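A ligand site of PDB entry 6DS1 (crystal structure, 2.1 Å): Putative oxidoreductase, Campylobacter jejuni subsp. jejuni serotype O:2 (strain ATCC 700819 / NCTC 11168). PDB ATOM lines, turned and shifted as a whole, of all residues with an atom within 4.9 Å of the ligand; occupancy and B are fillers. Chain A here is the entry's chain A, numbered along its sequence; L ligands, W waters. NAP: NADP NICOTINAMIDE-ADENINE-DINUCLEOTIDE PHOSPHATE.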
ATOM      1  N   GLY A  14     -25.104  10.925   3.923  1.00  0.00           N
ATOM      2  CA  GLY A  14     -25.243  12.358   3.711  1.00  0.00           C
ATOM      3  C   GLY A  14     -26.127  12.709   2.548  1.00  0.00           C
ATOM      4  O   GLY A  14     -26.028  13.811   2.007  1.00  0.00           O
ATOM      5  N   ALA A  16     -29.122  13.604   2.325  1.00  0.00           N
ATOM      6  CA  ALA A  16     -30.260  14.488   2.589  1.00  0.00           C
ATOM      7  C   ALA A  16     -30.058  15.893   2.048  1.00  0.00           C
ATOM      8  O   ALA A  16     -31.043  16.609   1.856  1.00  0.00           O
ATOM      9  CB  ALA A  16     -30.546  14.573   4.090  1.00  0.00           C
ATOM     10  N   LYS A  17     -28.814  16.315   1.824  1.00  0.00           N
ATOM     11  CA  LYS A  17     -28.529  17.681   1.377  1.00  0.00           C
ATOM     12  C   LYS A  17     -27.409  17.647   0.347  1.00  0.00           C
ATOM     13  O   LYS A  17     -26.675  16.662   0.230  1.00  0.00           O
ATOM     14  CB  LYS A  17     -28.103  18.597   2.535  1.00  0.00           C
ATOM     15  CG  LYS A  17     -29.071  18.653   3.706  1.00  0.00           C
ATOM     16  CD  LYS A  17     -28.528  19.564   4.816  1.00  0.00           C
ATOM     17  CE  LYS A  17     -29.482  19.611   6.005  1.00  0.00           C
ATOM     18  NZ  LYS A  17     -28.791  20.013   7.259  1.00  0.00           N
ATOM     19  N   GLY A  18     -27.309  18.755  -0.406  1.00  0.00           N
ATOM     20  CA  GLY A  18     -26.122  19.025  -1.209  1.00  0.00           C
ATOM     21  C   GLY A  18     -25.862  17.975  -2.273  1.00  0.00           C
ATOM     22  O   GLY A  18     -26.768  17.519  -2.971  1.00  0.00           O
ATOM     23  N   ILE A  19     -24.590  17.566  -2.390  1.00  0.00           N
ATOM     24  CA  ILE A  19     -24.181  16.648  -3.439  1.00  0.00           C
ATOM     25  C   ILE A  19     -24.946  15.326  -3.327  1.00  0.00           C
ATOM     26  O   ILE A  19     -25.545  14.854  -4.297  1.00  0.00           O
ATOM     27  CB  ILE A  19     -22.658  16.416  -3.392  1.00  0.00           C
ATOM     28  CG1 ILE A  19     -21.923  17.664  -3.894  1.00  0.00           C
ATOM     29  CG2 ILE A  19     -22.300  15.186  -4.188  1.00  0.00           C
ATOM     30  CD1 ILE A  19     -20.404  17.585  -3.750  1.00  0.00           C
ATOM     31  N   GLY A  20     -24.927  14.710  -2.137  1.00  0.00           N
ATOM     32  CA  GLY A  20     -25.590  13.431  -1.964  1.00  0.00           C
ATOM     33  C   GLY A  20     -27.074  13.489  -2.271  1.00  0.00           C
ATOM     34  O   GLY A  20     -27.643  12.517  -2.784  1.00  0.00           O
ATOM     35  N   PHE A  37     -28.942   7.702   4.458  1.00  0.00           N
ATOM     36  CA  PHE A  37     -28.407   7.702   5.816  1.00  0.00           C
ATOM     37  C   PHE A  37     -27.827   9.096   6.055  1.00  0.00           C
ATOM     38  O   PHE A  37     -26.865   9.474   5.374  1.00  0.00           O
ATOM     39  CB  PHE A  37     -27.285   6.666   6.013  1.00  0.00           C
ATOM     40  CG  PHE A  37     -27.734   5.227   6.097  1.00  0.00           C
ATOM     41  CD1 PHE A  37     -28.997   4.825   5.692  1.00  0.00           C
ATOM     42  CD2 PHE A  37     -26.858   4.259   6.585  1.00  0.00           C
ATOM     43  CE1 PHE A  37     -29.377   3.490   5.783  1.00  0.00           C
ATOM     44  CE2 PHE A  37     -27.226   2.930   6.674  1.00  0.00           C
ATOM     45  CZ  PHE A  37     -28.496   2.543   6.273  1.00  0.00           C
ATOM     46  N   SER A  38     -28.398   9.856   6.988  1.00  0.00           N
ATOM     47  CA  SER A  38     -27.892  11.196   7.253  1.00  0.00           C
ATOM     48  C   SER A  38     -28.435  11.658   8.608  1.00  0.00           C
ATOM     49  O   SER A  38     -29.307  11.017   9.197  1.00  0.00           O
ATOM     50  CB  SER A  38     -28.287  12.178   6.127  1.00  0.00           C
ATOM     51  OG  SER A  38     -27.467  13.333   6.129  1.00  0.00           O
ATOM     52  N   ARG A  39     -27.915  12.799   9.073  1.00  0.00           N
ATOM     53  CA  ARG A  39     -28.257  13.283  10.411  1.00  0.00           C
ATOM     54  C   ARG A  39     -29.708  13.736  10.529  1.00  0.00           C
ATOM     55  O   ARG A  39     -30.314  13.622  11.602  1.00  0.00           O
ATOM     56  CB  ARG A  39     -27.331  14.439  10.801  1.00  0.00           C
ATOM     57  CG  ARG A  39     -25.977  14.042  11.307  1.00  0.00           C
ATOM     58  CD  ARG A  39     -25.216  15.249  11.818  1.00  0.00           C
ATOM     59  NE  ARG A  39     -23.799  14.955  12.011  1.00  0.00           N
ATOM     60  CZ  ARG A  39     -22.820  15.463  11.274  1.00  0.00           C
ATOM     61  NH1 ARG A  39     -23.092  16.302  10.272  1.00  0.00           N
ATOM     62  NH2 ARG A  39     -21.556  15.139  11.537  1.00  0.00           N
ATOM     63  N   SER A  40     -30.268  14.264   9.451  1.00  0.00           N
ATOM     64  CA  SER A  40     -31.639  14.738   9.437  1.00  0.00           C
ATOM     65  C   SER A  40     -32.045  14.858   7.988  1.00  0.00           C
ATOM     66  O   SER A  40     -31.184  14.910   7.107  1.00  0.00           O
ATOM     67  CB  SER A  40     -31.791  16.094  10.139  1.00  0.00           C
ATOM     68  OG  SER A  40     -31.214  17.092   9.319  1.00  0.00           O
ATOM     69  N   ILE A  61     -29.215   9.056  11.301  1.00  0.00           N
ATOM     70  CA  ILE A  61     -28.024   8.591  12.003  1.00  0.00           C
ATOM     71  C   ILE A  61     -26.898   9.598  11.857  1.00  0.00           C
ATOM     72  O   ILE A  61     -26.720  10.190  10.792  1.00  0.00           O
ATOM     73  CB  ILE A  61     -27.560   7.216  11.483  1.00  0.00           C
ATOM     74  CG1 ILE A  61     -26.288   6.811  12.269  1.00  0.00           C
ATOM     75  CG2 ILE A  61     -27.380   7.228   9.959  1.00  0.00           C
ATOM     76  CD1 ILE A  61     -25.567   5.625  11.775  1.00  0.00           C
ATOM     77  N   ASP A  62     -26.118   9.770  12.929  1.00  0.00           N
ATOM     78  CA  ASP A  62     -24.824  10.438  12.856  1.00  0.00           C
ATOM     79  C   ASP A  62     -23.763   9.363  12.699  1.00  0.00           C
ATOM     80  O   ASP A  62     -23.522   8.589  13.635  1.00  0.00           O
ATOM     81  CB  ASP A  62     -24.564  11.289  14.098  1.00  0.00           C
ATOM     82  CG  ASP A  62     -23.317  12.176  13.933  1.00  0.00           C
ATOM     83  OD1 ASP A  62     -22.353  11.771  13.257  1.00  0.00           O
ATOM     84  OD2 ASP A  62     -23.285  13.268  14.511  1.00  0.00           O
ATOM     85  N   LEU A  63     -23.112   9.323  11.534  1.00  0.00           N
ATOM     86  CA  LEU A  63     -22.188   8.260  11.167  1.00  0.00           C
ATOM     87  C   LEU A  63     -20.865   8.307  11.935  1.00  0.00           C
ATOM     88  O   LEU A  63     -20.041   7.410  11.723  1.00  0.00           O
ATOM     89  CB  LEU A  63     -21.946   8.279   9.659  1.00  0.00           C
ATOM     90  CG  LEU A  63     -23.261   8.134   8.881  1.00  0.00           C
ATOM     91  CD1 LEU A  63     -23.154   8.645   7.457  1.00  0.00           C
ATOM     92  CD2 LEU A  63     -23.681   6.687   8.884  1.00  0.00           C
ATOM     93  N   LYS A  64     -20.636   9.294  12.805  1.00  0.00           N
ATOM     94  CA  LYS A  64     -19.538   9.142  13.752  1.00  0.00           C
ATOM     95  C   LYS A  64     -19.811   7.991  14.723  1.00  0.00           C
ATOM     96  O   LYS A  64     -18.876   7.364  15.210  1.00  0.00           O
ATOM     97  CB  LYS A  64     -19.293  10.471  14.495  1.00  0.00           C
ATOM     98  CG  LYS A  64     -20.283  10.813  15.592  1.00  0.00           C
ATOM     99  CD  LYS A  64     -19.869  12.092  16.334  1.00  0.00           C
ATOM    100  CE  LYS A  64     -20.745  12.326  17.582  1.00  0.00           C
ATOM    101  NZ  LYS A  64     -20.658  11.228  18.620  1.00  0.00           N
ATOM    102  N   ASN A  89     -20.685   9.442   0.991  1.00  0.00           N
ATOM    103  CA  ASN A  89     -20.668  10.858   0.651  1.00  0.00           C
ATOM    104  C   ASN A  89     -20.655  11.783   1.852  1.00  0.00           C
ATOM    105  O   ASN A  89     -20.218  12.933   1.718  1.00  0.00           O
ATOM    106  CB  ASN A  89     -21.874  11.174  -0.240  1.00  0.00           C
ATOM    107  CG  ASN A  89     -22.162  12.652  -0.359  1.00  0.00           C
ATOM    108  OD1 ASN A  89     -21.580  13.336  -1.193  1.00  0.00           O
ATOM    109  ND2 ASN A  89     -23.086  13.144   0.459  1.00  0.00           N
ATOM    110  N   ALA A  90     -21.091  11.330   3.031  1.00  0.00           N
ATOM    111  CA  ALA A  90     -21.166  12.202   4.188  1.00  0.00           C
ATOM    112  C   ALA A  90     -19.781  12.690   4.581  1.00  0.00           C
ATOM    113  O   ALA A  90     -18.847  11.890   4.715  1.00  0.00           O
ATOM    114  CB  ALA A  90     -21.816  11.463   5.367  1.00  0.00           C
ATOM    115  N   GLY A  91     -19.655  13.998   4.756  1.00  0.00           N
ATOM    116  CA  GLY A  91     -18.372  14.581   5.148  1.00  0.00           C
ATOM    117  C   GLY A  91     -18.493  16.078   5.317  1.00  0.00           C
ATOM    118  O   GLY A  91     -19.482  16.700   4.913  1.00  0.00           O
ATOM    119  N   THR A  92     -17.456  16.654   5.924  1.00  0.00           N
ATOM    120  CA  THR A  92     -17.399  18.087   6.210  1.00  0.00           C
ATOM    121  C   THR A  92     -15.950  18.537   6.133  1.00  0.00           C
ATOM    122  O   THR A  92     -15.100  17.993   6.837  1.00  0.00           O
ATOM    123  CB  THR A  92     -17.959  18.398   7.597  1.00  0.00           C
ATOM    124  OG1 THR A  92     -19.289  17.877   7.721  1.00  0.00           O
ATOM    125  CG2 THR A  92     -17.963  19.903   7.865  1.00  0.00           C
ATOM    126  N   ASN A 112     -16.005  11.886  12.213  1.00  0.00           N
ATOM    127  CA  ASN A 112     -17.048  12.546  11.422  1.00  0.00           C
ATOM    128  C   ASN A 112     -16.889  12.273   9.933  1.00  0.00           C
ATOM    129  O   ASN A 112     -17.896  12.223   9.218  1.00  0.00           O
ATOM    130  CB  ASN A 112     -17.034  14.058  11.667  1.00  0.00           C
ATOM    131  CG  ASN A 112     -17.230  14.419  13.145  1.00  0.00           C
ATOM    132  OD1 ASN A 112     -18.006  13.767  13.851  1.00  0.00           O
ATOM    133  ND2 ASN A 112     -16.567  15.477  13.588  1.00  0.00           N
ATOM    134  N   HIS A 116     -16.604   5.930   8.893  1.00  0.00           N
ATOM    135  CA  HIS A 116     -17.847   5.327   8.404  1.00  0.00           C
ATOM    136  C   HIS A 116     -17.787   4.968   6.919  1.00  0.00           C
ATOM    137  O   HIS A 116     -18.538   4.102   6.478  1.00  0.00           O
ATOM    138  CB  HIS A 116     -19.032   6.263   8.695  1.00  0.00           C
ATOM    139  CG  HIS A 116     -18.849   7.643   8.162  1.00  0.00           C
ATOM    140  ND1 HIS A 116     -19.093   7.970   6.839  1.00  0.00           N
ATOM    141  CD2 HIS A 116     -18.450   8.782   8.766  1.00  0.00           C
ATOM    142  CE1 HIS A 116     -18.845   9.254   6.666  1.00  0.00           C
ATOM    143  NE2 HIS A 116     -18.449   9.767   7.812  1.00  0.00           N
ATOM    144  N   TYR A 117     -16.893   5.590   6.131  1.00  0.00           N
ATOM    145  CA  TYR A 117     -16.667   5.094   4.772  1.00  0.00           C
ATOM    146  C   TYR A 117     -16.258   3.628   4.803  1.00  0.00           C
ATOM    147  O   TYR A 117     -16.671   2.837   3.944  1.00  0.00           O
ATOM    148  CB  TYR A 117     -15.565   5.889   4.067  1.00  0.00           C
ATOM    149  CG  TYR A 117     -16.022   7.134   3.346  1.00  0.00           C
ATOM    150  CD1 TYR A 117     -16.812   8.073   3.984  1.00  0.00           C
ATOM    151  CD2 TYR A 117     -15.606   7.396   2.039  1.00  0.00           C
ATOM    152  CE1 TYR A 117     -17.206   9.222   3.335  1.00  0.00           C
ATOM    153  CE2 TYR A 117     -16.004   8.552   1.376  1.00  0.00           C
ATOM    154  CZ  TYR A 117     -16.801   9.461   2.048  1.00  0.00           C
ATOM    155  OH  TYR A 117     -17.193  10.615   1.442  1.00  0.00           O
ATOM    156  N   ILE A 138     -17.265   9.613  -2.563  1.00  0.00           N
ATOM    157  CA  ILE A 138     -17.124  11.017  -2.902  1.00  0.00           C
ATOM    158  C   ILE A 138     -15.960  11.551  -2.085  1.00  0.00           C
ATOM    159  O   ILE A 138     -15.993  11.540  -0.850  1.00  0.00           O
ATOM    160  CB  ILE A 138     -18.416  11.785  -2.617  1.00  0.00           C
ATOM    161  CG1 ILE A 138     -19.632  11.111  -3.291  1.00  0.00           C
ATOM    162  CG2 ILE A 138     -18.253  13.263  -3.009  1.00  0.00           C
ATOM    163  CD1 ILE A 138     -19.601  11.069  -4.833  1.00  0.00           C
ATOM    164  N   VAL A 139     -14.889  11.964  -2.779  1.00  0.00           N
ATOM    165  CA  VAL A 139     -13.692  12.423  -2.089  1.00  0.00           C
ATOM    166  C   VAL A 139     -13.598  13.920  -2.354  1.00  0.00           C
ATOM    167  O   VAL A 139     -14.615  14.616  -2.310  1.00  0.00           O
ATOM    168  CB  VAL A 139     -12.438  11.627  -2.510  1.00  0.00           C
ATOM    169  CG1 VAL A 139     -12.597  10.175  -2.107  1.00  0.00           C
ATOM    170  CG2 VAL A 139     -12.184  11.703  -4.008  1.00  0.00           C
ATOM    171  N   SER A 140     -12.382  14.428  -2.587  1.00  0.00           N
ATOM    172  CA  SER A 140     -12.245  15.866  -2.788  1.00  0.00           C
ATOM    173  C   SER A 140     -10.919  16.165  -3.476  1.00  0.00           C
ATOM    174  O   SER A 140      -9.936  15.453  -3.275  1.00  0.00           O
ATOM    175  CB  SER A 140     -12.313  16.641  -1.466  1.00  0.00           C
ATOM    176  OG  SER A 140     -11.892  17.987  -1.667  1.00  0.00           O
ATOM    177  N   LYS A 141     -10.921  17.247  -4.275  1.00  0.00           N
ATOM    178  CA  LYS A 141      -9.670  17.745  -4.873  1.00  0.00           C
ATOM    179  C   LYS A 141      -8.565  17.836  -3.823  1.00  0.00           C
ATOM    180  O   LYS A 141      -7.412  17.475  -4.097  1.00  0.00           O
ATOM    181  CB  LYS A 141      -9.897  19.133  -5.507  1.00  0.00           C
ATOM    182  CG  LYS A 141      -9.655  20.314  -4.567  1.00  0.00           C
ATOM    183  CD  LYS A 141     -10.354  21.591  -5.003  1.00  0.00           C
ATOM    184  CE  LYS A 141     -10.769  22.467  -3.804  1.00  0.00           C
ATOM    185  NZ  LYS A 141     -11.960  21.943  -3.043  1.00  0.00           N
ATOM    186  N   TYR A 153      -9.048  17.136   6.966  1.00  0.00           N
ATOM    187  CA  TYR A 153      -9.918  16.873   5.813  1.00  0.00           C
ATOM    188  C   TYR A 153      -9.133  16.350   4.616  1.00  0.00           C
ATOM    189  O   TYR A 153      -9.609  15.459   3.903  1.00  0.00           O
ATOM    190  CB  TYR A 153     -10.670  18.141   5.451  1.00  0.00           C
ATOM    191  CG  TYR A 153     -11.578  18.037   4.234  1.00  0.00           C
ATOM    192  CD1 TYR A 153     -12.801  17.385   4.298  1.00  0.00           C
ATOM    193  CD2 TYR A 153     -11.205  18.628   3.029  1.00  0.00           C
ATOM    194  CE1 TYR A 153     -13.642  17.314   3.196  1.00  0.00           C
ATOM    195  CE2 TYR A 153     -12.034  18.563   1.926  1.00  0.00           C
ATOM    196  CZ  TYR A 153     -13.243  17.902   2.007  1.00  0.00           C
ATOM    197  OH  TYR A 153     -14.066  17.825   0.910  1.00  0.00           O
ATOM    198  N   LYS A 157      -9.720  12.503   2.963  1.00  0.00           N
ATOM    199  CA  LYS A 157     -10.110  12.361   1.554  1.00  0.00           C
ATOM    200  C   LYS A 157      -9.061  11.576   0.771  1.00  0.00           C
ATOM    201  O   LYS A 157      -9.413  10.730  -0.056  1.00  0.00           O
ATOM    202  CB  LYS A 157     -10.347  13.744   0.954  1.00  0.00           C
ATOM    203  CG  LYS A 157     -11.539  14.453   1.587  1.00  0.00           C
ATOM    204  CD  LYS A 157     -12.802  13.691   1.221  1.00  0.00           C
ATOM    205  CE  LYS A 157     -13.874  13.721   2.313  1.00  0.00           C
ATOM    206  NZ  LYS A 157     -15.165  13.176   1.781  1.00  0.00           N
ATOM    207  N   PRO A 183     -14.703  16.075  -6.427  1.00  0.00           N
ATOM    208  CA  PRO A 183     -15.138  17.413  -6.834  1.00  0.00           C
ATOM    209  C   PRO A 183     -14.137  18.450  -6.360  1.00  0.00           C
ATOM    210  O   PRO A 183     -13.341  18.214  -5.447  1.00  0.00           O
ATOM    211  CB  PRO A 183     -16.502  17.576  -6.136  1.00  0.00           C
ATOM    212  CG  PRO A 183     -16.853  16.216  -5.590  1.00  0.00           C
ATOM    213  CD  PRO A 183     -15.530  15.550  -5.333  1.00  0.00           C
ATOM    214  N   ALA A 184     -14.148  19.606  -7.039  1.00  0.00           N
ATOM    215  CA  ALA A 184     -13.315  20.722  -6.577  1.00  0.00           C
ATOM    216  C   ALA A 184     -14.166  21.739  -5.828  1.00  0.00           C
ATOM    217  O   ALA A 184     -14.120  21.825  -4.593  1.00  0.00           O
ATOM    218  CB  ALA A 184     -12.601  21.380  -7.757  1.00  0.00           C
ATOM    219  N   GLU A 185     -14.953  22.534  -6.558  1.00  0.00           N
ATOM    220  CA  GLU A 185     -15.856  23.499  -5.957  1.00  0.00           C
ATOM    221  C   GLU A 185     -17.247  23.260  -6.527  1.00  0.00           C
ATOM    222  O   GLU A 185     -17.432  23.346  -7.746  1.00  0.00           O
ATOM    223  CB  GLU A 185     -15.391  24.934  -6.236  1.00  0.00           C
ATOM    224  CG  GLU A 185     -13.961  25.200  -5.793  1.00  0.00           C
ATOM    225  CD  GLU A 185     -13.845  25.370  -4.278  1.00  0.00           C
ATOM    226  OE1 GLU A 185     -14.879  25.519  -3.597  1.00  0.00           O
ATOM    227  OE2 GLU A 185     -12.704  25.338  -3.764  1.00  0.00           O
ATOM    228  N   VAL A 186     -18.194  22.920  -5.651  1.00  0.00           N
ATOM    229  CA  VAL A 186     -19.570  22.586  -6.045  1.00  0.00           C
ATOM    230  C   VAL A 186     -20.526  23.498  -5.285  1.00  0.00           C
ATOM    231  O   VAL A 186     -20.537  23.491  -4.050  1.00  0.00           O
ATOM    232  CB  VAL A 186     -19.915  21.117  -5.770  1.00  0.00           C
ATOM    233  CG1 VAL A 186     -21.330  20.829  -6.255  1.00  0.00           C
ATOM    234  CG2 VAL A 186     -18.925  20.187  -6.429  1.00  0.00           C
ATOM    235  N   THR A 188     -23.662  24.503  -3.494  1.00  0.00           N
ATOM    236  CA  THR A 188     -24.751  23.913  -2.746  1.00  0.00           C
ATOM    237  C   THR A 188     -25.476  25.026  -2.011  1.00  0.00           C
ATOM    238  O   THR A 188     -24.965  26.150  -1.915  1.00  0.00           O
ATOM    239  CB  THR A 188     -24.226  22.890  -1.717  1.00  0.00           C
ATOM    240  OG1 THR A 188     -23.432  23.573  -0.750  1.00  0.00           O
ATOM    241  CG2 THR A 188     -23.403  21.799  -2.394  1.00  0.00           C
ATOM    242  N   LEU A 190     -25.711  25.156   1.172  1.00  0.00           N
ATOM    243  CA  LEU A 190     -24.871  25.464   2.323  1.00  0.00           C
ATOM    244  C   LEU A 190     -23.614  26.238   1.912  1.00  0.00           C
ATOM    245  O   LEU A 190     -23.154  27.106   2.666  1.00  0.00           O
ATOM    246  CB  LEU A 190     -24.529  24.166   3.064  1.00  0.00           C
ATOM    247  CG  LEU A 190     -25.705  23.696   3.946  1.00  0.00           C
ATOM    248  CD1 LEU A 190     -25.573  22.257   4.480  1.00  0.00           C
ATOM    249  CD2 LEU A 190     -25.898  24.676   5.095  1.00  0.00           C
ATOM    250  N   TYR A 191     -23.041  25.940   0.741  1.00  0.00           N
ATOM    251  CA  TYR A 191     -21.956  26.771   0.227  1.00  0.00           C
ATOM    252  C   TYR A 191     -22.436  28.203   0.015  1.00  0.00           C
ATOM    253  O   TYR A 191     -21.781  29.159   0.425  1.00  0.00           O
ATOM    254  CB  TYR A 191     -21.411  26.202  -1.080  1.00  0.00           C
ATOM    255  CG  TYR A 191     -19.930  26.461  -1.322  1.00  0.00           C
ATOM    256  CD1 TYR A 191     -19.354  27.709  -1.051  1.00  0.00           C
ATOM    257  CD2 TYR A 191     -19.108  25.454  -1.815  1.00  0.00           C
ATOM    258  CE1 TYR A 191     -18.005  27.938  -1.264  1.00  0.00           C
ATOM    259  CE2 TYR A 191     -17.760  25.666  -2.043  1.00  0.00           C
ATOM    260  CZ  TYR A 191     -17.207  26.914  -1.764  1.00  0.00           C
ATOM    261  OH  TYR A 191     -15.861  27.113  -1.997  1.00  0.00           O
HETATM  262  PA  NAP L   1     -23.297  19.422   2.463  1.00  0.00           P
HETATM  263  O1A NAP L   1     -24.135  20.151   1.436  1.00  0.00           O
HETATM  264  O2A NAP L   1     -23.018  19.987   3.834  1.00  0.00           O
HETATM  265  O5B NAP L   1     -23.997  18.003   2.681  1.00  0.00           O
HETATM  266  C5B NAP L   1     -23.360  17.010   3.458  1.00  0.00           C
HETATM  267  C4B NAP L   1     -24.421  16.067   3.969  1.00  0.00           C
HETATM  268  O4B NAP L   1     -23.773  15.028   4.701  1.00  0.00           O
HETATM  269  C3B NAP L   1     -25.332  16.785   4.942  1.00  0.00           C
HETATM  270  O3B NAP L   1     -26.651  16.244   4.824  1.00  0.00           O
HETATM  271  C2B NAP L   1     -24.799  16.425   6.306  1.00  0.00           C
HETATM  272  O2B NAP L   1     -25.846  16.479   7.281  1.00  0.00           O
HETATM  273  C1B NAP L   1     -24.305  15.016   6.014  1.00  0.00           C
HETATM  274  N9A NAP L   1     -23.276  14.521   6.951  1.00  0.00           N
HETATM  275  C8A NAP L   1     -22.011  14.950   7.079  1.00  0.00           C
HETATM  276  N7A NAP L   1     -21.353  14.251   8.047  1.00  0.00           N
HETATM  277  C5A NAP L   1     -22.222  13.337   8.549  1.00  0.00           C
HETATM  278  C6A NAP L   1     -22.195  12.295   9.587  1.00  0.00           C
HETATM  279  N6A NAP L   1     -21.065  12.051  10.304  1.00  0.00           N
HETATM  280  N1A NAP L   1     -23.331  11.572   9.782  1.00  0.00           N
HETATM  281  C2A NAP L   1     -24.460  11.783   9.068  1.00  0.00           C
HETATM  282  N3A NAP L   1     -24.566  12.725   8.108  1.00  0.00           N
HETATM  283  C4A NAP L   1     -23.492  13.523   7.817  1.00  0.00           C
HETATM  284  O3  NAP L   1     -21.873  18.985   1.872  1.00  0.00           O
HETATM  285  PN  NAP L   1     -21.510  18.614   0.354  1.00  0.00           P
HETATM  286  O1N NAP L   1     -20.771  19.812  -0.213  1.00  0.00           O
HETATM  287  O2N NAP L   1     -22.665  18.041  -0.412  1.00  0.00           O
HETATM  288  O5D NAP L   1     -20.438  17.459   0.664  1.00  0.00           O
HETATM  289  C5D NAP L   1     -20.705  16.065   0.454  1.00  0.00           C
HETATM  290  C4D NAP L   1     -19.393  15.448  -0.006  1.00  0.00           C
HETATM  291  O4D NAP L   1     -18.877  16.218  -1.084  1.00  0.00           O
HETATM  292  C3D NAP L   1     -18.346  15.488   1.093  1.00  0.00           C
HETATM  293  O3D NAP L   1     -17.804  14.178   1.270  1.00  0.00           O
HETATM  294  C2D NAP L   1     -17.258  16.407   0.573  1.00  0.00           C
HETATM  295  O2D NAP L   1     -15.952  15.917   0.916  1.00  0.00           O
HETATM  296  C1D NAP L   1     -17.482  16.408  -0.921  1.00  0.00           C
HETATM  297  N1N NAP L   1     -16.984  17.627  -1.573  1.00  0.00           N
HETATM  298  C2N NAP L   1     -17.754  18.716  -1.715  1.00  0.00           C
HETATM  299  C3N NAP L   1     -17.259  19.867  -2.337  1.00  0.00           C
HETATM  300  C7N NAP L   1     -18.110  21.099  -2.509  1.00  0.00           C
HETATM  301  O7N NAP L   1     -17.627  22.063  -3.072  1.00  0.00           O
HETATM  302  N7N NAP L   1     -19.374  21.103  -2.091  1.00  0.00           N
HETATM  303  C4N NAP L   1     -15.954  19.883  -2.814  1.00  0.00           C
HETATM  304  C5N NAP L   1     -15.176  18.746  -2.672  1.00  0.00           C
HETATM  305  C6N NAP L   1     -15.718  17.627  -2.037  1.00  0.00           C
HETATM  306  P2B NAP L   1     -26.112  17.747   8.259  1.00  0.00           P
HETATM  307  O1X NAP L   1     -25.732  18.968   7.448  1.00  0.00           O
HETATM  308  O2X NAP L   1     -27.601  17.632   8.514  1.00  0.00           O
HETATM  309  O3X NAP L   1     -25.267  17.501   9.480  1.00  0.00           O
HETATM  310  O   HOH W   1     -23.925  15.993   0.310  1.00  0.00           O
HETATM  311  O   HOH W   2     -28.684  15.551   6.905  1.00  0.00           O
HETATM  312  O   HOH W   3     -26.022  22.015   0.927  1.00  0.00           O
HETATM  313  O   HOH W   4     -21.473  22.751   3.636  1.00  0.00           O
HETATM  314  O   HOH W   5     -28.653  17.768  10.927  1.00  0.00           O
HETATM  315  O   HOH W   6     -18.661  15.194   8.728  1.00  0.00           O
HETATM  316  O   HOH W   7     -21.642  22.081   0.552  1.00  0.00           O
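The backbone NH (N) of Arg 39 lies within hydrogen-bond range of a nitrogen (N3A) of the ligand, at 3.5 Å.
NH1 of Arg 39 lies within salt-bridge range of O3X of the ligand.
An oxygen (O2D) of the ligand is in hydrogen-bond range of the side-chain hydroxyl of Tyr 153 (2.7 Å).
O3D of the ligand is in hydrogen-bond range of O of Asn 89 (2.8 Å).
The backbone NH (N) of Val 186 lies within hydrogen-bond range of an oxygen (O7N) of the ligand, at 2.8 Å.
O of Val 186 sits at hydrogen-bond distance from N7N of the ligand, 3.3 Å away.
An oxygen (O2N) of the ligand is in hydrogen-bond range of the backbone NH of Ile 19 (2.8 Å).
A nitrogen (N1A) of the ligand lies within hydrogen-bond range of the backbone NH of Leu 63, at 2.9 Å.
O3D of the ligand sits at hydrogen-bond distance from NZ of Lys 157, 2.9 Å away.
The side-chain amino group (NZ) of Lys 17 is in salt-bridge range of an oxygen (O2X) of the ligand (2.9 Å).
N6A of the ligand sits at hydrogen-bond distance from OD1 of Asp 62.
The side-chain hydroxyl (OG) of Ser 38 sits at hydrogen-bond distance from an oxygen (O3B) of the ligand (3.3 Å).
The backbone carbonyl oxygen (O) of Asn 112 lies within hydrogen-bond range of a nitrogen (N6A) of the ligand.
NE of Arg 39 is in salt-bridge range of OD2 of Asp 62.
The backbone NH (N) of Arg 39 is in hydrogen-bond range of the backbone carbonyl oxygen (O) of Ile 61 (3.3 Å).
NZ of Lys 157 is in hydrogen-bond range of OH of Tyr 117.
N of Gly 14 sits at hydrogen-bond distance from O of Phe 37, 2.7 Å away.
The backbone carbonyl oxygen (O) of Ala 184 sits at hydrogen-bond distance from the side-chain amino group (NZ) of Lys 141, at 2.7 Å.
The backbone NH (N) of Ile 61 is in hydrogen-bond range of the backbone carbonyl oxygen (O) of Ser 38, 2.9 Å away.
The backbone NH (N) of Leu 190 sits close to the side-chain hydroxyl (OG1) of Thr 188, 3.4 Å away.
OH of Tyr 191 sits at hydrogen-bond distance from OE1 of Glu 185 (2.5 Å).
Merely in contact with the ligand: Gly 14, Gly 18, Ser 40, Ile 61, Lys 64, Ala 90, Gly 91, Tyr 117, Ile 138, Val 139, Ser 140, Pro 183, Ala 184, Glu 185, Thr 188, Leu 190 and Tyr 191.
Hydrophobic or aromatic side chains within 4 Å of the ligand: Ile 19, Leu 63, Ala 90, Ile 138, Tyr 153, Pro 183, Val 186, Leu 190 and Tyr 191.
28 residues have an atom within 4 Å of the ligand: Gly 14, Lys 17, Gly 18, Ile 19, Ser 38, Arg 39, Ser 40, Ile 61, Asp 62, Leu 63, Lys 64, Asn 89, Ala 90, Gly 91, Asn 112, Tyr 117, Ile 138, Val 139, Ser 140, Tyr 153, Lys 157, Pro 183, Ala 184, Glu 185, Val 186, Thr 188, Leu 190 and Tyr 191.
The nearest printed residue that does not touch the ligand is Thr 92 (4.05 Å).
Water W7 bridges O1N of the ligand (2.5 Å) and OG1 of Thr 188 (2.7 Å).
Water W5 lies within hydrogen-bond range of an oxygen (O2X) of the ligand (2.6 Å) and the side-chain hydroxyl (OG) of Ser 40 (3.1 Å).
Water W3 lies within hydrogen-bond range of O1A of the ligand, N of Leu 190 and OG1 of Thr 188.
Water W2 lies within hydrogen-bond range of the backbone carbonyl oxygen (O) of Ser 40 (2.6 Å), the side-chain hydroxyl (OG) of Ser 38 (2.6 Å) and an oxygen (O2X) of the ligand (2.8 Å).
Water W6 lies within hydrogen-bond range of N7A of the ligand, OG1 of Thr 92 and O of Asn 112.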
